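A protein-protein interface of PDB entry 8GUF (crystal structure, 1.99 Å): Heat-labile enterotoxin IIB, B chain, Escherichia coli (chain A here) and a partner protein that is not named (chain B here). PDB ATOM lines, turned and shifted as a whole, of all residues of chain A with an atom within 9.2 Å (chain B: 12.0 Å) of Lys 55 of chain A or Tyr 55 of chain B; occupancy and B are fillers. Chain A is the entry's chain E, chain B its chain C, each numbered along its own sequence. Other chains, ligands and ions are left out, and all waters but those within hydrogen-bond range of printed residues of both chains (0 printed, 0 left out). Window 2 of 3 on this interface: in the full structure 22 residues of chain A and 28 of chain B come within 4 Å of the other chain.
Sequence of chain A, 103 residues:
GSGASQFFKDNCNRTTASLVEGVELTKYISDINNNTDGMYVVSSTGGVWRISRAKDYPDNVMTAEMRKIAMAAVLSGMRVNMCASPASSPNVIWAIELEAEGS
OD1 of Asp 37 of chain A sits close to OD1 of Asp 57 of chain B (2.6 Å). The backbone NH of Ala 54 of chain A sits at hydrogen-bond distance from the side-chain hydroxyl of Tyr 55 of chain B, at 3.2 Å. The side-chain carboxylate of Glu 63 of chain B is in salt-bridge range of the guanidinium group of Arg 67 of chain A, at 3.4 Å.
The backbone carbonyl oxygen of Lys 55 of chain A is in hydrogen-bond range of the side-chain amide nitrogen of Asn 60 of chain A (3.3 Å). O of Thr 63 of chain A sits at hydrogen-bond distance from NH1 of Arg 67 of chain A (3.4 Å). N of Tyr 55 of chain B lies close to ND2 of Asn 58 of chain B (3.4 Å). OG1 of Thr 61 of chain B lies within hydrogen-bond range of O of Asp 57 of chain B.
CG of Pro 56 of chain B touches OD2 of Asp 37 of chain A (3.7 Å). Met 60 of chain B touches Asp 37 of chain A (CE to OD2, 3.2 Å). Tyr 55 of chain B touches Arg 53 of chain A. Arg 53 of chain A touches Pro 56 of chain B. Lys 55 of chain A touches Tyr 55 of chain B (N to CZ, 3.5 Å). Arg 67 of chain A touches Val 59 of chain B.
Lys 55 of chain A touches just one residue of chain B: Tyr 55 (3.5 Å). Tyr 55 of chain B touches three residues of chain A. Arg 53 of chain A touches two residues of chain B. No residue of chain B comes within 4 Å of Asn 60 of chain A. Printed residues of chain A within 4 Å of Pro 56 of chain B: Asp 37 and Arg 53. Printed residues of chain A within 4 Å of Asp 57 of chain B: Asp 37. Of the printed residues of chain A, Glu 63 of chain B touches Arg 67. Of the printed residues of chain A, Val 59 of chain B touches Arg 67. Printed residues of chain B within 4 Å of Asp 37 of chain A: Pro 56 (3.7 Å), Asp 57 (2.6 Å) and Met 60 (3.2 Å). Printed residues of chain A within 4 Å of Met 60 of chain B: Asp 37. Ala 62 of chain B touches none of the printed residues of chain A. The nearest residue of chain A that does not touch Tyr 55 of chain B is Asp 56 of chain A (6.0 Å). The nearest printed residue of chain B that does not touch Asp 37 of chain A is Tyr 55 of chain B (7.0 Å).
Printed residues of chain A that touch a printed residue of chain B: Asp 37, Arg 53, Ala 54, Lys 55 and Arg 67. Among the printed residues, 9 pairs touch across the chains. Among the printed residues, Asp or Glu carboxylates within 4 Å of a Lys or Arg side-chain nitrogen of the other chain: Arg 67 of chain A with Glu 63 of chain B (3.4 Å).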
ATOM      1  N   ASP A  37      12.637 -25.293  -3.083  1.00  0.00           N
ATOM      2  CA  ASP A  37      11.639 -25.053  -2.056  1.00  0.00           C
ATOM      3  C   ASP A  37      10.480 -24.263  -2.654  1.00  0.00           C
ATOM      4  O   ASP A  37      10.689 -23.178  -3.172  1.00  0.00           O
ATOM      5  CB  ASP A  37      12.334 -24.287  -0.918  1.00  0.00           C
ATOM      6  CG  ASP A  37      11.526 -24.133   0.350  1.00  0.00           C
ATOM      7  OD1 ASP A  37      11.285 -25.166   1.017  1.00  0.00           O
ATOM      8  OD2 ASP A  37      11.122 -22.985   0.639  1.00  0.00           O
ATOM      9  N   ILE A  51       3.853 -20.908  -7.479  1.00  0.00           N
ATOM     10  CA  ILE A  51       2.776 -20.143  -6.862  1.00  0.00           C
ATOM     11  C   ILE A  51       3.406 -19.110  -5.922  1.00  0.00           C
ATOM     12  O   ILE A  51       4.357 -19.435  -5.223  1.00  0.00           O
ATOM     13  CB  ILE A  51       1.810 -21.087  -6.120  1.00  0.00           C
ATOM     14  CG1 ILE A  51       1.246 -22.178  -7.038  1.00  0.00           C
ATOM     15  CG2 ILE A  51       0.715 -20.289  -5.441  1.00  0.00           C
ATOM     16  CD1 ILE A  51       0.336 -23.155  -6.324  1.00  0.00           C
ATOM     17  N   SER A  52       2.940 -17.855  -5.959  1.00  0.00           N
ATOM     18  CA  SER A  52       3.441 -16.832  -5.043  1.00  0.00           C
ATOM     19  C   SER A  52       3.240 -17.260  -3.579  1.00  0.00           C
ATOM     20  O   SER A  52       2.365 -18.075  -3.245  1.00  0.00           O
ATOM     21  CB  SER A  52       2.785 -15.509  -5.303  1.00  0.00           C
ATOM     22  OG  SER A  52       3.208 -14.973  -6.543  1.00  0.00           O
ATOM     23  N   ARG A  53       4.077 -16.715  -2.694  1.00  0.00           N
ATOM     24  CA  ARG A  53       3.827 -16.885  -1.272  1.00  0.00           C
ATOM     25  C   ARG A  53       4.128 -15.571  -0.560  1.00  0.00           C
ATOM     26  O   ARG A  53       4.827 -14.729  -1.123  1.00  0.00           O
ATOM     27  CB  ARG A  53       4.635 -18.064  -0.733  1.00  0.00           C
ATOM     28  CG  ARG A  53       6.132 -17.891  -0.916  1.00  0.00           C
ATOM     29  CD  ARG A  53       6.857 -19.114  -0.420  1.00  0.00           C
ATOM     30  NE  ARG A  53       8.265 -18.816  -0.245  1.00  0.00           N
ATOM     31  CZ  ARG A  53       9.249 -19.333  -0.966  1.00  0.00           C
ATOM     32  NH1 ARG A  53       9.001 -20.131  -2.003  1.00  0.00           N
ATOM     33  NH2 ARG A  53      10.490 -19.014  -0.636  1.00  0.00           N
ATOM     34  N   ALA A  54       3.496 -15.402   0.611  1.00  0.00           N
ATOM     35  CA  ALA A  54       3.643 -14.241   1.486  1.00  0.00           C
ATOM     36  C   ALA A  54       3.370 -14.678   2.930  1.00  0.00           C
ATOM     37  O   ALA A  54       2.486 -15.491   3.162  1.00  0.00           O
ATOM     38  CB  ALA A  54       2.695 -13.146   1.051  1.00  0.00           C
ATOM     39  N   LYS A  55       4.133 -14.173   3.904  1.00  0.00           N
ATOM     40  CA  LYS A  55       3.864 -14.530   5.291  1.00  0.00           C
ATOM     41  C   LYS A  55       2.849 -13.547   5.877  1.00  0.00           C
ATOM     42  O   LYS A  55       2.028 -13.926   6.713  1.00  0.00           O
ATOM     43  CB  LYS A  55       5.151 -14.611   6.117  1.00  0.00           C
ATOM     44  CG  LYS A  55       5.356 -13.524   7.161  1.00  0.00           C
ATOM     45  CD  LYS A  55       6.483 -13.823   8.135  1.00  0.00           C
ATOM     46  CE  LYS A  55       7.859 -13.566   7.562  1.00  0.00           C
ATOM     47  NZ  LYS A  55       8.892 -13.648   8.620  1.00  0.00           N
ATOM     48  N   ASP A  56       2.845 -12.306   5.379  1.00  0.00           N
ATOM     49  CA  ASP A  56       2.092 -11.246   6.029  1.00  0.00           C
ATOM     50  C   ASP A  56       0.695 -11.099   5.446  1.00  0.00           C
ATOM     51  O   ASP A  56       0.478 -11.298   4.249  1.00  0.00           O
ATOM     52  CB  ASP A  56       2.791  -9.898   5.895  1.00  0.00           C
ATOM     53  CG  ASP A  56       3.887  -9.697   6.914  1.00  0.00           C
ATOM     54  OD1 ASP A  56       4.306 -10.701   7.537  1.00  0.00           O
ATOM     55  OD2 ASP A  56       4.276  -8.533   7.103  1.00  0.00           O
ATOM     56  N   TYR A  57      -0.228 -10.712   6.334  1.00  0.00           N
ATOM     57  CA  TYR A  57      -1.536 -10.211   5.949  1.00  0.00           C
ATOM     58  C   TYR A  57      -1.293  -8.948   5.109  1.00  0.00           C
ATOM     59  O   TYR A  57      -0.385  -8.192   5.391  1.00  0.00           O
ATOM     60  CB  TYR A  57      -2.421 -10.031   7.199  1.00  0.00           C
ATOM     61  CG  TYR A  57      -3.770  -9.411   6.935  1.00  0.00           C
ATOM     62  CD1 TYR A  57      -3.937  -8.037   6.908  1.00  0.00           C
ATOM     63  CD2 TYR A  57      -4.881 -10.197   6.639  1.00  0.00           C
ATOM     64  CE1 TYR A  57      -5.170  -7.459   6.619  1.00  0.00           C
ATOM     65  CE2 TYR A  57      -6.121  -9.641   6.378  1.00  0.00           C
ATOM     66  CZ  TYR A  57      -6.264  -8.264   6.367  1.00  0.00           C
ATOM     67  OH  TYR A  57      -7.469  -7.693   6.064  1.00  0.00           O
ATOM     68  N   PRO A  58      -2.054  -8.677   4.035  1.00  0.00           N
ATOM     69  CA  PRO A  58      -3.113  -9.577   3.577  1.00  0.00           C
ATOM     70  C   PRO A  58      -2.744 -10.590   2.496  1.00  0.00           C
ATOM     71  O   PRO A  58      -3.574 -11.402   2.105  1.00  0.00           O
ATOM     72  CB  PRO A  58      -4.143  -8.581   3.047  1.00  0.00           C
ATOM     73  CG  PRO A  58      -3.367  -7.380   2.573  1.00  0.00           C
ATOM     74  CD  PRO A  58      -2.038  -7.404   3.300  1.00  0.00           C
ATOM     75  N   ASP A  59      -1.492 -10.585   2.041  1.00  0.00           N
ATOM     76  CA  ASP A  59      -1.128 -11.407   0.897  1.00  0.00           C
ATOM     77  C   ASP A  59      -1.031 -12.880   1.309  1.00  0.00           C
ATOM     78  O   ASP A  59      -1.125 -13.767   0.466  1.00  0.00           O
ATOM     79  CB  ASP A  59       0.121 -10.841   0.219  1.00  0.00           C
ATOM     80  CG  ASP A  59      -0.165  -9.665  -0.704  1.00  0.00           C
ATOM     81  OD1 ASP A  59      -1.349  -9.357  -0.939  1.00  0.00           O
ATOM     82  OD2 ASP A  59       0.802  -9.086  -1.210  1.00  0.00           O
ATOM     83  N   ASN A  60      -0.871 -13.141   2.608  1.00  0.00           N
ATOM     84  CA  ASN A  60      -0.893 -14.501   3.128  1.00  0.00           C
ATOM     85  C   ASN A  60      -2.244 -15.163   2.856  1.00  0.00           C
ATOM     86  O   ASN A  60      -2.295 -16.377   2.672  1.00  0.00           O
ATOM     87  CB  ASN A  60      -0.490 -14.553   4.611  1.00  0.00           C
ATOM     88  CG  ASN A  60      -1.497 -13.925   5.552  1.00  0.00           C
ATOM     89  OD1 ASN A  60      -2.463 -13.307   5.136  1.00  0.00           O
ATOM     90  ND2 ASN A  60      -1.297 -14.094   6.844  1.00  0.00           N
ATOM     91  N   VAL A  61      -3.311 -14.357   2.774  1.00  0.00           N
ATOM     92  CA  VAL A  61      -4.640 -14.809   2.416  1.00  0.00           C
ATOM     93  C   VAL A  61      -4.697 -15.134   0.920  1.00  0.00           C
ATOM     94  O   VAL A  61      -5.078 -16.246   0.563  1.00  0.00           O
ATOM     95  CB  VAL A  61      -5.737 -13.803   2.827  1.00  0.00           C
ATOM     96  CG1 VAL A  61      -7.086 -14.132   2.206  1.00  0.00           C
ATOM     97  CG2 VAL A  61      -5.896 -13.680   4.331  1.00  0.00           C
ATOM     98  N   THR A  63      -2.404 -15.673  -1.276  1.00  0.00           N
ATOM     99  CA  THR A  63      -1.535 -16.751  -1.706  1.00  0.00           C
ATOM    100  C   THR A  63      -2.107 -18.090  -1.230  1.00  0.00           C
ATOM    101  O   THR A  63      -1.993 -19.089  -1.926  1.00  0.00           O
ATOM    102  CB  THR A  63      -0.086 -16.525  -1.283  1.00  0.00           C
ATOM    103  OG1 THR A  63      -0.069 -16.372   0.133  1.00  0.00           O
ATOM    104  CG2 THR A  63       0.529 -15.327  -1.960  1.00  0.00           C
ATOM    105  N   ALA A  64      -2.746 -18.125  -0.065  1.00  0.00           N
ATOM    106  CA  ALA A  64      -3.389 -19.360   0.369  1.00  0.00           C
ATOM    107  C   ALA A  64      -4.534 -19.707  -0.583  1.00  0.00           C
ATOM    108  O   ALA A  64      -4.765 -20.876  -0.838  1.00  0.00           O
ATOM    109  CB  ALA A  64      -3.885 -19.258   1.798  1.00  0.00           C
ATOM    110  N   ARG A  67      -3.260 -21.366  -3.786  1.00  0.00           N
ATOM    111  CA  ARG A  67      -3.040 -22.791  -3.570  1.00  0.00           C
ATOM    112  C   ARG A  67      -4.363 -23.576  -3.664  1.00  0.00           C
ATOM    113  O   ARG A  67      -4.421 -24.657  -4.270  1.00  0.00           O
ATOM    114  CB  ARG A  67      -2.283 -22.979  -2.249  1.00  0.00           C
ATOM    115  CG  ARG A  67      -0.873 -22.404  -2.289  1.00  0.00           C
ATOM    116  CD  ARG A  67      -0.007 -22.770  -1.108  1.00  0.00           C
ATOM    117  NE  ARG A  67      -0.636 -22.336   0.123  1.00  0.00           N
ATOM    118  CZ  ARG A  67      -0.339 -21.208   0.750  1.00  0.00           C
ATOM    119  NH1 ARG A  67       0.425 -20.290   0.164  1.00  0.00           N
ATOM    120  NH2 ARG A  67      -0.814 -21.020   1.973  1.00  0.00           N
ATOM    121  N   ARG B  51       7.239 -31.959   8.284  1.00  0.00           N
ATOM    122  CA  ARG B  51       6.560 -30.834   8.903  1.00  0.00           C
ATOM    123  C   ARG B  51       7.576 -29.748   9.275  1.00  0.00           C
ATOM    124  O   ARG B  51       8.755 -30.012   9.399  1.00  0.00           O
ATOM    125  CB  ARG B  51       5.748 -31.309  10.111  1.00  0.00           C
ATOM    126  CG  ARG B  51       6.593 -31.987  11.182  1.00  0.00           C
ATOM    127  CD  ARG B  51       5.945 -31.972  12.559  1.00  0.00           C
ATOM    128  NE  ARG B  51       6.889 -32.224  13.653  1.00  0.00           N
ATOM    129  CZ  ARG B  51       7.327 -33.423  14.000  1.00  0.00           C
ATOM    130  NH1 ARG B  51       6.868 -34.493  13.368  1.00  0.00           N
ATOM    131  NH2 ARG B  51       8.214 -33.540  14.977  1.00  0.00           N
ATOM    132  N   ALA B  52       7.061 -28.554   9.552  1.00  0.00           N
ATOM    133  CA  ALA B  52       7.844 -27.347   9.742  1.00  0.00           C
ATOM    134  C   ALA B  52       6.956 -26.343  10.458  1.00  0.00           C
ATOM    135  O   ALA B  52       5.811 -26.188  10.048  1.00  0.00           O
ATOM    136  CB  ALA B  52       8.273 -26.802   8.397  1.00  0.00           C
ATOM    137  N   LYS B  53       7.477 -25.694  11.516  1.00  0.00           N
ATOM    138  CA  LYS B  53       6.713 -24.741  12.309  1.00  0.00           C
ATOM    139  C   LYS B  53       6.564 -23.434  11.550  1.00  0.00           C
ATOM    140  O   LYS B  53       5.535 -22.797  11.627  1.00  0.00           O
ATOM    141  CB  LYS B  53       7.365 -24.328  13.648  1.00  0.00           C
ATOM    142  CG  LYS B  53       8.212 -23.036  13.615  1.00  0.00           C
ATOM    143  CD  LYS B  53       8.710 -22.405  14.949  1.00  0.00           C
ATOM    144  CE  LYS B  53       8.816 -23.409  16.068  1.00  0.00           C
ATOM    145  NZ  LYS B  53       7.475 -23.959  16.383  1.00  0.00           N
ATOM    146  N   ASP B  54       7.603 -23.019  10.840  1.00  0.00           N
ATOM    147  CA  ASP B  54       7.722 -21.626  10.462  1.00  0.00           C
ATOM    148  C   ASP B  54       7.699 -21.501   8.943  1.00  0.00           C
ATOM    149  O   ASP B  54       7.951 -22.464   8.228  1.00  0.00           O
ATOM    150  CB  ASP B  54       8.977 -20.969  11.055  1.00  0.00           C
ATOM    151  CG  ASP B  54       9.015 -19.466  10.805  1.00  0.00           C
ATOM    152  OD1 ASP B  54       7.935 -18.795  10.989  1.00  0.00           O
ATOM    153  OD2 ASP B  54      10.106 -18.965  10.381  1.00  0.00           O
ATOM    154  N   TYR B  55       7.410 -20.266   8.528  1.00  0.00           N
ATOM    155  CA  TYR B  55       7.375 -19.801   7.154  1.00  0.00           C
ATOM    156  C   TYR B  55       8.767 -19.922   6.528  1.00  0.00           C
ATOM    157  O   TYR B  55       9.769 -19.606   7.172  1.00  0.00           O
ATOM    158  CB  TYR B  55       6.863 -18.357   7.148  1.00  0.00           C
ATOM    159  CG  TYR B  55       6.742 -17.738   5.773  1.00  0.00           C
ATOM    160  CD1 TYR B  55       5.627 -17.991   4.972  1.00  0.00           C
ATOM    161  CD2 TYR B  55       7.726 -16.898   5.266  1.00  0.00           C
ATOM    162  CE1 TYR B  55       5.510 -17.424   3.714  1.00  0.00           C
ATOM    163  CE2 TYR B  55       7.634 -16.337   3.995  1.00  0.00           C
ATOM    164  CZ  TYR B  55       6.510 -16.591   3.224  1.00  0.00           C
ATOM    165  OH  TYR B  55       6.373 -16.047   1.970  1.00  0.00           O
ATOM    166  N   PRO B  56       8.897 -20.329   5.243  1.00  0.00           N
ATOM    167  CA  PRO B  56       7.763 -20.709   4.385  1.00  0.00           C
ATOM    168  C   PRO B  56       7.372 -22.186   4.340  1.00  0.00           C
ATOM    169  O   PRO B  56       6.390 -22.550   3.701  1.00  0.00           O
ATOM    170  CB  PRO B  56       8.277 -20.302   2.995  1.00  0.00           C
ATOM    171  CG  PRO B  56       9.780 -20.530   3.065  1.00  0.00           C
ATOM    172  CD  PRO B  56      10.170 -20.280   4.507  1.00  0.00           C
ATOM    173  N   ASP B  57       8.129 -23.050   5.011  1.00  0.00           N
ATOM    174  CA  ASP B  57       7.908 -24.484   4.870  1.00  0.00           C
ATOM    175  C   ASP B  57       6.652 -24.971   5.614  1.00  0.00           C
ATOM    176  O   ASP B  57       6.137 -26.061   5.325  1.00  0.00           O
ATOM    177  CB  ASP B  57       9.166 -25.237   5.289  1.00  0.00           C
ATOM    178  CG  ASP B  57      10.219 -25.195   4.208  1.00  0.00           C
ATOM    179  OD1 ASP B  57       9.891 -24.719   3.118  1.00  0.00           O
ATOM    180  OD2 ASP B  57      11.312 -25.700   4.451  1.00  0.00           O
ATOM    181  N   ASN B  58       6.133 -24.185   6.564  1.00  0.00           N
ATOM    182  CA  ASN B  58       4.828 -24.498   7.129  1.00  0.00           C
ATOM    183  C   ASN B  58       3.752 -24.484   6.038  1.00  0.00           C
ATOM    184  O   ASN B  58       2.801 -25.261   6.107  1.00  0.00           O
ATOM    185  CB  ASN B  58       4.426 -23.598   8.301  1.00  0.00           C
ATOM    186  CG  ASN B  58       4.400 -22.102   8.046  1.00  0.00           C
ATOM    187  OD1 ASN B  58       4.547 -21.599   6.934  1.00  0.00           O
ATOM    188  ND2 ASN B  58       4.216 -21.362   9.131  1.00  0.00           N
ATOM    189  N   VAL B  59       3.917 -23.652   5.006  1.00  0.00           N
ATOM    190  CA  VAL B  59       3.017 -23.723   3.866  1.00  0.00           C
ATOM    191  C   VAL B  59       3.199 -25.053   3.143  1.00  0.00           C
ATOM    192  O   VAL B  59       2.221 -25.767   2.911  1.00  0.00           O
ATOM    193  CB  VAL B  59       3.204 -22.550   2.893  1.00  0.00           C
ATOM    194  CG1 VAL B  59       2.457 -22.801   1.592  1.00  0.00           C
ATOM    195  CG2 VAL B  59       2.781 -21.233   3.519  1.00  0.00           C
ATOM    196  N   MET B  60       4.437 -25.358   2.728  1.00  0.00           N
ATOM    197  CA  MET B  60       4.652 -26.504   1.865  1.00  0.00           C
ATOM    198  C   MET B  60       4.240 -27.797   2.585  1.00  0.00           C
ATOM    199  O   MET B  60       3.647 -28.688   1.966  1.00  0.00           O
ATOM    200  CB  MET B  60       6.118 -26.590   1.402  1.00  0.00           C
ATOM    201  CG  MET B  60       6.413 -25.838   0.102  1.00  0.00           C
ATOM    202  SD  MET B  60       6.331 -24.040   0.214  1.00  0.00           S
ATOM    203  CE  MET B  60       8.017 -23.682   0.701  1.00  0.00           C
ATOM    204  N   THR B  61       4.515 -27.899   3.896  1.00  0.00           N
ATOM    205  CA  THR B  61       4.199 -29.118   4.625  1.00  0.00           C
ATOM    206  C   THR B  61       2.683 -29.255   4.803  1.00  0.00           C
ATOM    207  O   THR B  61       2.161 -30.356   4.701  1.00  0.00           O
ATOM    208  CB  THR B  61       5.020 -29.233   5.920  1.00  0.00           C
ATOM    209  OG1 THR B  61       4.781 -28.057   6.683  1.00  0.00           O
ATOM    210  CG2 THR B  61       6.498 -29.395   5.629  1.00  0.00           C
ATOM    211  N   ALA B  62       1.975 -28.137   4.996  1.00  0.00           N
ATOM    212  CA  ALA B  62       0.523 -28.175   5.046  1.00  0.00           C
ATOM    213  C   ALA B  62      -0.032 -28.696   3.709  1.00  0.00           C
ATOM    214  O   ALA B  62      -0.967 -29.489   3.682  1.00  0.00           O
ATOM    215  CB  ALA B  62       0.002 -26.803   5.387  1.00  0.00           C
ATOM    216  N   GLU B  63       0.551 -28.268   2.585  1.00  0.00           N
ATOM    217  CA  GLU B  63       0.094 -28.729   1.274  1.00  0.00           C
ATOM    218  C   GLU B  63       0.412 -30.206   1.042  1.00  0.00           C
ATOM    219  O   GLU B  63      -0.369 -30.904   0.372  1.00  0.00           O
ATOM    220  CB  GLU B  63       0.682 -27.861   0.161  1.00  0.00           C
ATOM    221  CG  GLU B  63       0.246 -26.391   0.201  1.00  0.00           C
ATOM    222  CD  GLU B  63      -1.253 -26.166   0.296  1.00  0.00           C
ATOM    223  OE1 GLU B  63      -1.966 -26.773  -0.512  1.00  0.00           O
ATOM    224  OE2 GLU B  63      -1.702 -25.381   1.175  1.00  0.00           O
ATOM    225  N   ARG B  65       0.281 -32.506   3.336  1.00  0.00           N
ATOM    226  CA  ARG B  65      -0.821 -33.117   4.066  1.00  0.00           C
ATOM    227  C   ARG B  65      -2.106 -33.080   3.232  1.00  0.00           C
ATOM    228  O   ARG B  65      -2.804 -34.091   3.146  1.00  0.00           O
ATOM    229  CB  ARG B  65      -1.006 -32.481   5.456  1.00  0.00           C
ATOM    230  CG  ARG B  65       0.184 -32.720   6.377  1.00  0.00           C
ATOM    231  CD  ARG B  65      -0.080 -32.316   7.824  1.00  0.00           C
ATOM    232  NE  ARG B  65      -0.327 -30.891   7.996  1.00  0.00           N
ATOM    233  CZ  ARG B  65       0.591 -29.934   8.148  1.00  0.00           C
ATOM    234  NH1 ARG B  65       1.882 -30.203   8.162  1.00  0.00           N
ATOM    235  NH2 ARG B  65       0.190 -28.690   8.289  1.00  0.00           N
